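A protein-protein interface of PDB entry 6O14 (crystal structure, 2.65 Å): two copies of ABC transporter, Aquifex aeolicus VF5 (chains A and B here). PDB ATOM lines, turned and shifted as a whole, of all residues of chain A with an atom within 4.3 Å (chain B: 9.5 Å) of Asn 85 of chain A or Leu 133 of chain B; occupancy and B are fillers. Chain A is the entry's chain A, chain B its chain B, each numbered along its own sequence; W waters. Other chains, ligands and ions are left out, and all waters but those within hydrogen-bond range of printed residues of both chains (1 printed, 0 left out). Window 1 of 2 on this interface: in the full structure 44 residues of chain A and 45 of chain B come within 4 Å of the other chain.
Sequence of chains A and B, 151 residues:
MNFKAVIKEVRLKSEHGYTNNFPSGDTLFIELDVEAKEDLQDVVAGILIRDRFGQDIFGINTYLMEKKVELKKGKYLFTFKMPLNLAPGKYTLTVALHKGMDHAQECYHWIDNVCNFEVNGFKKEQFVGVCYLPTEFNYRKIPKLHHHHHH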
ATOM      1  N   GLY A  25     -10.947 -17.741  12.412  1.00  0.00           N
ATOM      2  CA  GLY A  25     -10.999 -17.231  13.764  1.00  0.00           C
ATOM      3  C   GLY A  25     -10.397 -18.137  14.818  1.00  0.00           C
ATOM      4  O   GLY A  25     -10.188 -17.679  15.950  1.00  0.00           O
ATOM      5  N   ILE A  49       2.239 -14.797   6.255  1.00  0.00           N
ATOM      6  CA  ILE A  49       1.179 -15.607   5.671  1.00  0.00           C
ATOM      7  C   ILE A  49       0.856 -15.063   4.287  1.00  0.00           C
ATOM      8  O   ILE A  49       0.780 -13.841   4.079  1.00  0.00           O
ATOM      9  CB  ILE A  49      -0.067 -15.600   6.558  1.00  0.00           C
ATOM     10  CG1 ILE A  49       0.296 -16.048   7.981  1.00  0.00           C
ATOM     11  CG2 ILE A  49      -1.116 -16.492   5.947  1.00  0.00           C
ATOM     12  CD1 ILE A  49      -0.844 -15.863   8.970  1.00  0.00           C
ATOM     13  N   PHE A  58      -0.507 -11.241   5.715  1.00  0.00           N
ATOM     14  CA  PHE A  58      -0.060 -10.661   6.973  1.00  0.00           C
ATOM     15  C   PHE A  58       1.339 -11.135   7.332  1.00  0.00           C
ATOM     16  O   PHE A  58       1.618 -12.338   7.297  1.00  0.00           O
ATOM     17  CB  PHE A  58      -1.041 -11.016   8.089  1.00  0.00           C
ATOM     18  CG  PHE A  58      -0.537 -10.691   9.455  1.00  0.00           C
ATOM     19  CD1 PHE A  58      -0.403  -9.372   9.858  1.00  0.00           C
ATOM     20  CD2 PHE A  58      -0.192 -11.704  10.341  1.00  0.00           C
ATOM     21  CE1 PHE A  58       0.066  -9.071  11.121  1.00  0.00           C
ATOM     22  CE2 PHE A  58       0.277 -11.420  11.603  1.00  0.00           C
ATOM     23  CZ  PHE A  58       0.404 -10.104  11.995  1.00  0.00           C
ATOM     24  N   MET A  82      -1.781 -15.977  17.279  1.00  0.00           N
ATOM     25  CA  MET A  82      -2.603 -14.978  16.589  1.00  0.00           C
ATOM     26  C   MET A  82      -3.951 -15.547  16.175  1.00  0.00           C
ATOM     27  O   MET A  82      -4.020 -16.709  15.752  1.00  0.00           O
ATOM     28  CB  MET A  82      -1.893 -14.437  15.343  1.00  0.00           C
ATOM     29  CG  MET A  82      -2.049 -15.320  14.123  1.00  0.00           C
ATOM     30  SD  MET A  82      -0.691 -15.126  12.947  1.00  0.00           S
ATOM     31  CE  MET A  82       0.709 -15.234  14.068  1.00  0.00           C
ATOM     32  N   PRO A  83      -5.033 -14.767  16.250  1.00  0.00           N
ATOM     33  CA  PRO A  83      -6.316 -15.240  15.705  1.00  0.00           C
ATOM     34  C   PRO A  83      -6.226 -15.347  14.196  1.00  0.00           C
ATOM     35  O   PRO A  83      -5.762 -14.425  13.518  1.00  0.00           O
ATOM     36  CB  PRO A  83      -7.312 -14.156  16.123  1.00  0.00           C
ATOM     37  CG  PRO A  83      -6.484 -12.941  16.331  1.00  0.00           C
ATOM     38  CD  PRO A  83      -5.130 -13.399  16.785  1.00  0.00           C
ATOM     39  N   LEU A  84      -6.690 -16.476  13.668  1.00  0.00           N
ATOM     40  CA  LEU A  84      -6.699 -16.688  12.226  1.00  0.00           C
ATOM     41  C   LEU A  84      -7.941 -16.042  11.598  1.00  0.00           C
ATOM     42  O   LEU A  84      -8.761 -16.696  10.956  1.00  0.00           O
ATOM     43  CB  LEU A  84      -6.648 -18.180  11.943  1.00  0.00           C
ATOM     44  CG  LEU A  84      -5.827 -18.543  10.720  1.00  0.00           C
ATOM     45  CD1 LEU A  84      -4.666 -17.587  10.631  1.00  0.00           C
ATOM     46  CD2 LEU A  84      -5.340 -19.965  10.851  1.00  0.00           C
ATOM     47  N   ASN A  85      -8.029 -14.713  11.732  1.00  0.00           N
ATOM     48  CA  ASN A  85      -9.175 -13.956  11.223  1.00  0.00           C
ATOM     49  C   ASN A  85      -9.125 -13.778   9.693  1.00  0.00           C
ATOM     50  O   ASN A  85      -9.153 -12.667   9.164  1.00  0.00           O
ATOM     51  CB  ASN A  85      -9.230 -12.609  11.935  1.00  0.00           C
ATOM     52  CG  ASN A  85      -9.574 -12.738  13.419  1.00  0.00           C
ATOM     53  OD1 ASN A  85     -10.242 -13.689  13.828  1.00  0.00           O
ATOM     54  ND2 ASN A  85      -9.125 -11.768  14.231  1.00  0.00           N
ATOM     55  N   LEU A  86      -9.073 -14.902   8.971  1.00  0.00           N
ATOM     56  CA  LEU A  86      -8.872 -14.905   7.523  1.00  0.00           C
ATOM     57  C   LEU A  86      -9.965 -15.712   6.834  1.00  0.00           C
ATOM     58  O   LEU A  86     -10.460 -16.703   7.376  1.00  0.00           O
ATOM     59  CB  LEU A  86      -7.488 -15.491   7.138  1.00  0.00           C
ATOM     60  CG  LEU A  86      -6.282 -14.748   7.735  1.00  0.00           C
ATOM     61  CD1 LEU A  86      -4.934 -15.396   7.383  1.00  0.00           C
ATOM     62  CD2 LEU A  86      -6.311 -13.278   7.339  1.00  0.00           C
ATOM     63  N   LYS A 124     -16.263 -18.112  14.380  1.00  0.00           N
ATOM     64  CA  LYS A 124     -17.041 -16.921  14.687  1.00  0.00           C
ATOM     65  C   LYS A 124     -18.138 -16.786  13.622  1.00  0.00           C
ATOM     66  O   LYS A 124     -18.511 -17.770  12.980  1.00  0.00           O
ATOM     67  CB  LYS A 124     -16.100 -15.714  14.800  1.00  0.00           C
ATOM     68  CG  LYS A 124     -15.096 -15.829  15.965  1.00  0.00           C
ATOM     69  CD  LYS A 124     -14.163 -14.601  16.084  1.00  0.00           C
ATOM     70  CE  LYS A 124     -12.702 -14.942  15.747  1.00  0.00           C
ATOM     71  NZ  LYS A 124     -11.726 -14.712  16.861  1.00  0.00           N
ATOM     72  N   CYS A 131     -10.319 -10.849   4.966  1.00  0.00           N
ATOM     73  CA  CYS A 131     -10.096 -10.884   6.402  1.00  0.00           C
ATOM     74  C   CYS A 131     -11.387 -10.574   7.154  1.00  0.00           C
ATOM     75  O   CYS A 131     -12.353 -10.042   6.595  1.00  0.00           O
ATOM     76  CB  CYS A 131      -8.960  -9.925   6.784  1.00  0.00           C
ATOM     77  SG  CYS A 131      -9.428  -8.212   6.616  1.00  0.00           S
ATOM     78  N   TYR A 132     -11.355 -10.865   8.455  1.00  0.00           N
ATOM     79  CA  TYR A 132     -12.484 -10.692   9.361  1.00  0.00           C
ATOM     80  C   TYR A 132     -12.139  -9.692  10.459  1.00  0.00           C
ATOM     81  O   TYR A 132     -11.148  -9.868  11.174  1.00  0.00           O
ATOM     82  CB  TYR A 132     -12.882 -12.041   9.968  1.00  0.00           C
ATOM     83  CG  TYR A 132     -13.690 -11.955  11.252  1.00  0.00           C
ATOM     84  CD1 TYR A 132     -15.012 -11.528  11.238  1.00  0.00           C
ATOM     85  CD2 TYR A 132     -13.147 -12.349  12.467  1.00  0.00           C
ATOM     86  CE1 TYR A 132     -15.761 -11.471  12.398  1.00  0.00           C
ATOM     87  CE2 TYR A 132     -13.890 -12.302  13.630  1.00  0.00           C
ATOM     88  CZ  TYR A 132     -15.189 -11.860  13.586  1.00  0.00           C
ATOM     89  OH  TYR A 132     -15.925 -11.806  14.738  1.00  0.00           O
ATOM     90  N   SER B  24      -4.059   2.665  11.319  1.00  0.00           N
ATOM     91  CA  SER B  24      -4.426   1.263  11.249  1.00  0.00           C
ATOM     92  C   SER B  24      -4.600   0.700  12.655  1.00  0.00           C
ATOM     93  O   SER B  24      -3.767   0.915  13.549  1.00  0.00           O
ATOM     94  CB  SER B  24      -3.366   0.482  10.493  1.00  0.00           C
ATOM     95  OG  SER B  24      -3.679  -0.903  10.459  1.00  0.00           O
ATOM     96  N   GLY B  25      -5.694  -0.042  12.851  1.00  0.00           N
ATOM     97  CA  GLY B  25      -6.029  -0.568  14.157  1.00  0.00           C
ATOM     98  C   GLY B  25      -6.927   0.299  15.007  1.00  0.00           C
ATOM     99  O   GLY B  25      -7.420  -0.178  16.036  1.00  0.00           O
ATOM    100  N   ILE B  57     -12.479  -6.579   0.966  1.00  0.00           N
ATOM    101  CA  ILE B  57     -11.627  -6.797   2.127  1.00  0.00           C
ATOM    102  C   ILE B  57     -12.402  -7.382   3.292  1.00  0.00           C
ATOM    103  O   ILE B  57     -11.952  -8.347   3.918  1.00  0.00           O
ATOM    104  CB  ILE B  57     -10.926  -5.494   2.507  1.00  0.00           C
ATOM    105  CG1 ILE B  57      -9.876  -5.234   1.450  1.00  0.00           C
ATOM    106  CG2 ILE B  57     -10.281  -5.606   3.897  1.00  0.00           C
ATOM    107  CD1 ILE B  57      -9.567  -3.819   1.370  1.00  0.00           C
ATOM    108  N   PHE B  58     -13.575  -6.826   3.592  1.00  0.00           N
ATOM    109  CA  PHE B  58     -14.395  -7.373   4.664  1.00  0.00           C
ATOM    110  C   PHE B  58     -15.819  -6.864   4.539  1.00  0.00           C
ATOM    111  O   PHE B  58     -16.038  -5.676   4.282  1.00  0.00           O
ATOM    112  CB  PHE B  58     -13.848  -7.012   6.047  1.00  0.00           C
ATOM    113  CG  PHE B  58     -14.829  -7.260   7.150  1.00  0.00           C
ATOM    114  CD1 PHE B  58     -15.155  -8.557   7.521  1.00  0.00           C
ATOM    115  CD2 PHE B  58     -15.442  -6.198   7.804  1.00  0.00           C
ATOM    116  CE1 PHE B  58     -16.068  -8.804   8.550  1.00  0.00           C
ATOM    117  CE2 PHE B  58     -16.372  -6.422   8.822  1.00  0.00           C
ATOM    118  CZ  PHE B  58     -16.678  -7.732   9.200  1.00  0.00           C
ATOM    119  N   PRO B  83     -12.481  -2.891  14.831  1.00  0.00           N
ATOM    120  CA  PRO B  83     -11.083  -2.471  14.642  1.00  0.00           C
ATOM    121  C   PRO B  83     -10.726  -2.449  13.168  1.00  0.00           C
ATOM    122  O   PRO B  83     -11.037  -3.386  12.428  1.00  0.00           O
ATOM    123  CB  PRO B  83     -10.280  -3.545  15.383  1.00  0.00           C
ATOM    124  CG  PRO B  83     -11.164  -4.755  15.391  1.00  0.00           C
ATOM    125  CD  PRO B  83     -12.570  -4.189  15.528  1.00  0.00           C
ATOM    126  N   LEU B  84     -10.077  -1.372  12.741  1.00  0.00           N
ATOM    127  CA  LEU B  84      -9.617  -1.257  11.357  1.00  0.00           C
ATOM    128  C   LEU B  84      -8.231  -1.903  11.226  1.00  0.00           C
ATOM    129  O   LEU B  84      -7.205  -1.249  11.023  1.00  0.00           O
ATOM    130  CB  LEU B  84      -9.628   0.201  10.913  1.00  0.00           C
ATOM    131  CG  LEU B  84     -10.149   0.575   9.511  1.00  0.00           C
ATOM    132  CD1 LEU B  84     -11.279  -0.313   9.022  1.00  0.00           C
ATOM    133  CD2 LEU B  84     -10.580   2.024   9.491  1.00  0.00           C
ATOM    134  N   ASN B  85      -8.212  -3.227  11.401  1.00  0.00           N
ATOM    135  CA  ASN B  85      -6.989  -4.019  11.264  1.00  0.00           C
ATOM    136  C   ASN B  85      -6.650  -4.224   9.783  1.00  0.00           C
ATOM    137  O   ASN B  85      -6.509  -5.341   9.294  1.00  0.00           O
ATOM    138  CB  ASN B  85      -7.146  -5.356  11.975  1.00  0.00           C
ATOM    139  CG  ASN B  85      -7.476  -5.198  13.457  1.00  0.00           C
ATOM    140  OD1 ASN B  85      -7.038  -4.241  14.102  1.00  0.00           O
ATOM    141  ND2 ASN B  85      -8.250  -6.140  14.001  1.00  0.00           N
ATOM    142  N   LEU B  86      -6.499  -3.107   9.074  1.00  0.00           N
ATOM    143  CA  LEU B  86      -6.333  -3.097   7.627  1.00  0.00           C
ATOM    144  C   LEU B  86      -5.046  -2.373   7.274  1.00  0.00           C
ATOM    145  O   LEU B  86      -4.615  -1.458   7.985  1.00  0.00           O
ATOM    146  CB  LEU B  86      -7.511  -2.397   6.916  1.00  0.00           C
ATOM    147  CG  LEU B  86      -8.877  -3.057   7.098  1.00  0.00           C
ATOM    148  CD1 LEU B  86      -9.891  -2.474   6.143  1.00  0.00           C
ATOM    149  CD2 LEU B  86      -8.775  -4.557   6.914  1.00  0.00           C
ATOM    150  N   ALA B  87      -4.433  -2.783   6.170  1.00  0.00           N
ATOM    151  CA  ALA B  87      -3.209  -2.129   5.736  1.00  0.00           C
ATOM    152  C   ALA B  87      -3.471  -0.654   5.434  1.00  0.00           C
ATOM    153  O   ALA B  87      -4.586  -0.272   5.057  1.00  0.00           O
ATOM    154  CB  ALA B  87      -2.640  -2.817   4.497  1.00  0.00           C
ATOM    155  N   LYS B 124      -1.342   0.478  16.322  1.00  0.00           N
ATOM    156  CA  LYS B 124      -0.673  -0.672  16.916  1.00  0.00           C
ATOM    157  C   LYS B 124       0.716  -0.821  16.281  1.00  0.00           C
ATOM    158  O   LYS B 124       1.351   0.167  15.898  1.00  0.00           O
ATOM    159  CB  LYS B 124      -1.566  -1.910  16.757  1.00  0.00           C
ATOM    160  CG  LYS B 124      -2.885  -1.807  17.526  1.00  0.00           C
ATOM    161  CD  LYS B 124      -3.902  -2.873  17.108  1.00  0.00           C
ATOM    162  CE  LYS B 124      -5.317  -2.452  17.525  1.00  0.00           C
ATOM    163  NZ  LYS B 124      -6.426  -3.076  16.743  1.00  0.00           N
ATOM    164  N   GLU B 125       1.263  -2.034  16.301  1.00  0.00           N
ATOM    165  CA  GLU B 125       2.502  -2.315  15.591  1.00  0.00           C
ATOM    166  C   GLU B 125       2.346  -2.095  14.083  1.00  0.00           C
ATOM    167  O   GLU B 125       1.250  -1.926  13.540  1.00  0.00           O
ATOM    168  CB  GLU B 125       2.950  -3.755  15.826  1.00  0.00           C
ATOM    169  CG  GLU B 125       2.836  -4.198  17.265  1.00  0.00           C
ATOM    170  CD  GLU B 125       1.471  -4.750  17.557  1.00  0.00           C
ATOM    171  OE1 GLU B 125       0.873  -5.323  16.621  1.00  0.00           O
ATOM    172  OE2 GLU B 125       0.987  -4.590  18.702  1.00  0.00           O
ATOM    173  N   GLN B 126       3.485  -2.082  13.412  1.00  0.00           N
ATOM    174  CA  GLN B 126       3.506  -2.176  11.973  1.00  0.00           C
ATOM    175  C   GLN B 126       3.407  -3.626  11.544  1.00  0.00           C
ATOM    176  O   GLN B 126       3.770  -4.546  12.276  1.00  0.00           O
ATOM    177  CB  GLN B 126       4.780  -1.590  11.410  1.00  0.00           C
ATOM    178  CG  GLN B 126       5.004  -0.200  11.835  1.00  0.00           C
ATOM    179  CD  GLN B 126       6.122   0.411  11.051  1.00  0.00           C
ATOM    180  OE1 GLN B 126       6.492  -0.100   9.984  1.00  0.00           O
ATOM    181  NE2 GLN B 126       6.673   1.512  11.559  1.00  0.00           N
ATOM    182  N   PHE B 127       2.912  -3.817  10.331  1.00  0.00           N
ATOM    183  CA  PHE B 127       2.775  -5.140   9.759  1.00  0.00           C
ATOM    184  C   PHE B 127       2.841  -4.959   8.256  1.00  0.00           C
ATOM    185  O   PHE B 127       2.857  -3.836   7.758  1.00  0.00           O
ATOM    186  CB  PHE B 127       1.465  -5.802  10.187  1.00  0.00           C
ATOM    187  CG  PHE B 127       0.266  -5.041   9.746  1.00  0.00           C
ATOM    188  CD1 PHE B 127      -0.157  -3.933  10.454  1.00  0.00           C
ATOM    189  CD2 PHE B 127      -0.403  -5.392   8.583  1.00  0.00           C
ATOM    190  CE1 PHE B 127      -1.236  -3.200  10.038  1.00  0.00           C
ATOM    191  CE2 PHE B 127      -1.492  -4.662   8.156  1.00  0.00           C
ATOM    192  CZ  PHE B 127      -1.908  -3.559   8.887  1.00  0.00           C
ATOM    193  N   VAL B 128       2.936  -6.074   7.537  1.00  0.00           N
ATOM    194  CA  VAL B 128       2.800  -6.087   6.089  1.00  0.00           C
ATOM    195  C   VAL B 128       1.579  -6.920   5.737  1.00  0.00           C
ATOM    196  O   VAL B 128       1.046  -7.662   6.571  1.00  0.00           O
ATOM    197  CB  VAL B 128       4.049  -6.609   5.342  1.00  0.00           C
ATOM    198  CG1 VAL B 128       5.177  -5.628   5.492  1.00  0.00           C
ATOM    199  CG2 VAL B 128       4.435  -7.995   5.812  1.00  0.00           C
ATOM    200  N   GLY B 129       1.110  -6.757   4.480  1.00  0.00           N
ATOM    201  CA  GLY B 129      -0.030  -7.513   4.001  1.00  0.00           C
ATOM    202  C   GLY B 129      -1.326  -6.748   4.158  1.00  0.00           C
ATOM    203  O   GLY B 129      -1.378  -5.614   4.653  1.00  0.00           O
ATOM    204  N   VAL B 130      -2.407  -7.392   3.710  1.00  0.00           N
ATOM    205  CA  VAL B 130      -3.700  -6.716   3.637  1.00  0.00           C
ATOM    206  C   VAL B 130      -4.204  -6.352   5.028  1.00  0.00           C
ATOM    207  O   VAL B 130      -4.607  -5.210   5.284  1.00  0.00           O
ATOM    208  CB  VAL B 130      -4.719  -7.594   2.895  1.00  0.00           C
ATOM    209  CG1 VAL B 130      -6.135  -7.057   3.144  1.00  0.00           C
ATOM    210  CG2 VAL B 130      -4.395  -7.634   1.412  1.00  0.00           C
ATOM    211  N   CYS B 131      -4.215  -7.321   5.938  1.00  0.00           N
ATOM    212  CA  CYS B 131      -4.842  -7.176   7.242  1.00  0.00           C
ATOM    213  C   CYS B 131      -3.805  -7.338   8.351  1.00  0.00           C
ATOM    214  O   CYS B 131      -2.648  -7.700   8.119  1.00  0.00           O
ATOM    215  CB  CYS B 131      -5.984  -8.174   7.418  1.00  0.00           C
ATOM    216  SG  CYS B 131      -5.454  -9.846   7.137  1.00  0.00           S
ATOM    217  N   TYR B 132      -4.219  -7.021   9.570  1.00  0.00           N
ATOM    218  CA  TYR B 132      -3.372  -7.184  10.741  1.00  0.00           C
ATOM    219  C   TYR B 132      -4.023  -8.179  11.692  1.00  0.00           C
ATOM    220  O   TYR B 132      -5.152  -7.970  12.152  1.00  0.00           O
ATOM    221  CB  TYR B 132      -3.152  -5.838  11.417  1.00  0.00           C
ATOM    222  CG  TYR B 132      -2.702  -5.907  12.855  1.00  0.00           C
ATOM    223  CD1 TYR B 132      -3.622  -6.048  13.885  1.00  0.00           C
ATOM    224  CD2 TYR B 132      -1.365  -5.780  13.187  1.00  0.00           C
ATOM    225  CE1 TYR B 132      -3.220  -6.084  15.196  1.00  0.00           C
ATOM    226  CE2 TYR B 132      -0.956  -5.808  14.493  1.00  0.00           C
ATOM    227  CZ  TYR B 132      -1.886  -5.962  15.499  1.00  0.00           C
ATOM    228  OH  TYR B 132      -1.483  -5.998  16.814  1.00  0.00           O
ATOM    229  N   LEU B 133      -3.318  -9.260  11.983  1.00  0.00           N
ATOM    230  CA  LEU B 133      -3.773 -10.178  13.005  1.00  0.00           C
ATOM    231  C   LEU B 133      -3.002  -9.851  14.273  1.00  0.00           C
ATOM    232  O   LEU B 133      -1.762  -9.824  14.237  1.00  0.00           O
ATOM    233  CB  LEU B 133      -3.546 -11.624  12.573  1.00  0.00           C
ATOM    234  CG  LEU B 133      -4.094 -11.966  11.182  1.00  0.00           C
ATOM    235  CD1 LEU B 133      -3.431 -13.194  10.606  1.00  0.00           C
ATOM    236  CD2 LEU B 133      -5.611 -12.175  11.216  1.00  0.00           C
ATOM    237  N   PRO B 134      -3.664  -9.482  15.364  1.00  0.00           N
ATOM    238  CA  PRO B 134      -2.933  -9.220  16.615  1.00  0.00           C
ATOM    239  C   PRO B 134      -2.099 -10.428  17.013  1.00  0.00           C
ATOM    240  O   PRO B 134      -2.598 -11.550  17.074  1.00  0.00           O
ATOM    241  CB  PRO B 134      -4.048  -8.932  17.628  1.00  0.00           C
ATOM    242  CG  PRO B 134      -5.324  -9.421  16.963  1.00  0.00           C
ATOM    243  CD  PRO B 134      -5.112  -9.261  15.498  1.00  0.00           C
ATOM    244  N   THR B 135      -0.815 -10.202  17.271  1.00  0.00           N
ATOM    245  CA  THR B 135       0.117 -11.306  17.450  1.00  0.00           C
ATOM    246  C   THR B 135       0.857 -11.218  18.776  1.00  0.00           C
ATOM    247  O   THR B 135       1.213 -10.133  19.239  1.00  0.00           O
ATOM    248  CB  THR B 135       1.124 -11.335  16.290  1.00  0.00           C
ATOM    249  OG1 THR B 135       0.421 -11.161  15.056  1.00  0.00           O
ATOM    250  CG2 THR B 135       1.911 -12.644  16.246  1.00  0.00           C
ATOM    251  N   GLU B 136       1.046 -12.371  19.400  1.00  0.00           N
ATOM    252  CA  GLU B 136       1.874 -12.496  20.584  1.00  0.00           C
ATOM    253  C   GLU B 136       3.015 -13.441  20.249  1.00  0.00           C
ATOM    254  O   GLU B 136       2.855 -14.349  19.423  1.00  0.00           O
ATOM    255  CB  GLU B 136       1.080 -13.024  21.761  1.00  0.00           C
ATOM    256  CG  GLU B 136       0.074 -12.043  22.315  1.00  0.00           C
ATOM    257  CD  GLU B 136      -0.825 -12.684  23.352  1.00  0.00           C
ATOM    258  OE1 GLU B 136      -2.042 -12.389  23.329  1.00  0.00           O
ATOM    259  OE2 GLU B 136      -0.325 -13.478  24.188  1.00  0.00           O
HETATM  260  O   HOH W   1      -8.413  -8.815  12.808  1.00  0.00           O
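N of Ile 49 of chain A lies within hydrogen-bond range of O of Phe 58 of chain A, 2.7 Å away. O of Asn 85 of chain A sits at hydrogen-bond distance from N of Tyr 132 of chain A. The backbone carbonyl oxygen (O) of Leu 86 of chain B is in hydrogen-bond range of the side-chain hydroxyl (OG) of Ser 24 of chain B, 2.7 Å away. The backbone NH (N) of Tyr 132 of chain B sits at hydrogen-bond distance from the backbone carbonyl oxygen (O) of Asn 85 of chain B, 2.9 Å away. The side-chain carboxylate (OE1) of Glu 125 of chain B is in hydrogen-bond range of the side-chain hydroxyl (OH) of Tyr 132 of chain B, 2.5 Å away. The side-chain hydroxyl of Thr 135 of chain B sits at hydrogen-bond distance from the backbone carbonyl oxygen of Leu 133 of chain B (2.7 Å).
O of Ile 57 of chain B is in hydrogen-bond range of N of Cys 131 of chain A, 3.2 Å away.
Water W1 lies within hydrogen-bond range of the side-chain amide nitrogen of Asn 85 of chain B (2.9 Å), the side-chain amide nitrogen of Asn 85 of chain A (3.4 Å), the backbone carbonyl oxygen of Tyr 132 of chain A (3.4 Å) and the backbone carbonyl oxygen of Tyr 132 of chain B (3.4 Å).
Phe 58 of chain A touches Cys 131 of chain B, and with the chains exchanged Cys 131 of chain A touches Phe 58 of chain B. Phe 58 of chain A touches Tyr 132 of chain B, and with the chains exchanged Tyr 132 of chain A touches Phe 58 of chain B. Leu 86 of chain A touches Cys 131 of chain B, and with the chains exchanged Cys 131 of chain A touches Leu 86 of chain B. Cys 131 of chain A touches its own counterpart, Cys 131 of chain B. 9 positions are printed for both chains.
Val 128 of chain B touches Phe 58 of chain A. CD1 of Phe 58 of chain A touches O of Cys 131 of chain B, at 3.3 Å. Phe 58 of chain A touches Tyr 132 of chain B (CD1 to CA, 3.8 Å). Phe 58 of chain A touches Leu 133 of chain B. CZ of Phe 58 of chain A touches OG1 of Thr 135 of chain B (3.2 Å). Pro 134 of chain B touches Met 82 of chain A. Cys 131 of chain B touches Leu 86 of chain A (SG to CD2, 3.5 Å). Phe 58 of chain B touches Cys 131 of chain A. Cys 131 of chain A touches Cys 131 of chain B (CB to CB, 3.5 Å). Phe 58 of chain B touches Tyr 132 of chain A.
Gly 25 of chain A touches none of the printed residues of chain B. Pro 83 of chain A touches two residues of chain B. Of the printed residues of chain B, Asn 85 of chain A touches Leu 133 (3.5 Å). Of the printed residues of chain A, Ile 57 of chain B touches Cys 131. Of the printed residues of chain A, Leu 86 of chain B touches Cys 131 (3.7 Å). Glu 125 of chain B touches none of the printed residues of chain A. Printed residues of chain A within 4 Å of Tyr 132 of chain B: Phe 58. Leu 133 of chain B touches three residues of chain A. Of the printed residues of chain A, Thr 135 of chain B touches Phe 58 (3.2 Å) and Met 82 (3.6 Å). The nearest printed residue of chain A that does not touch Leu 133 of chain B is Ile 49 of chain A (4.1 Å).
Hydrophobic or aromatic side chains of chain A that line the printed part of chain B: Phe 58, Met 82, Pro 83, Leu 86 and Tyr 132. Among the printed residues, no Asp or Glu carboxylate lies within 4 Å of a Lys or Arg side-chain nitrogen of the other chain.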
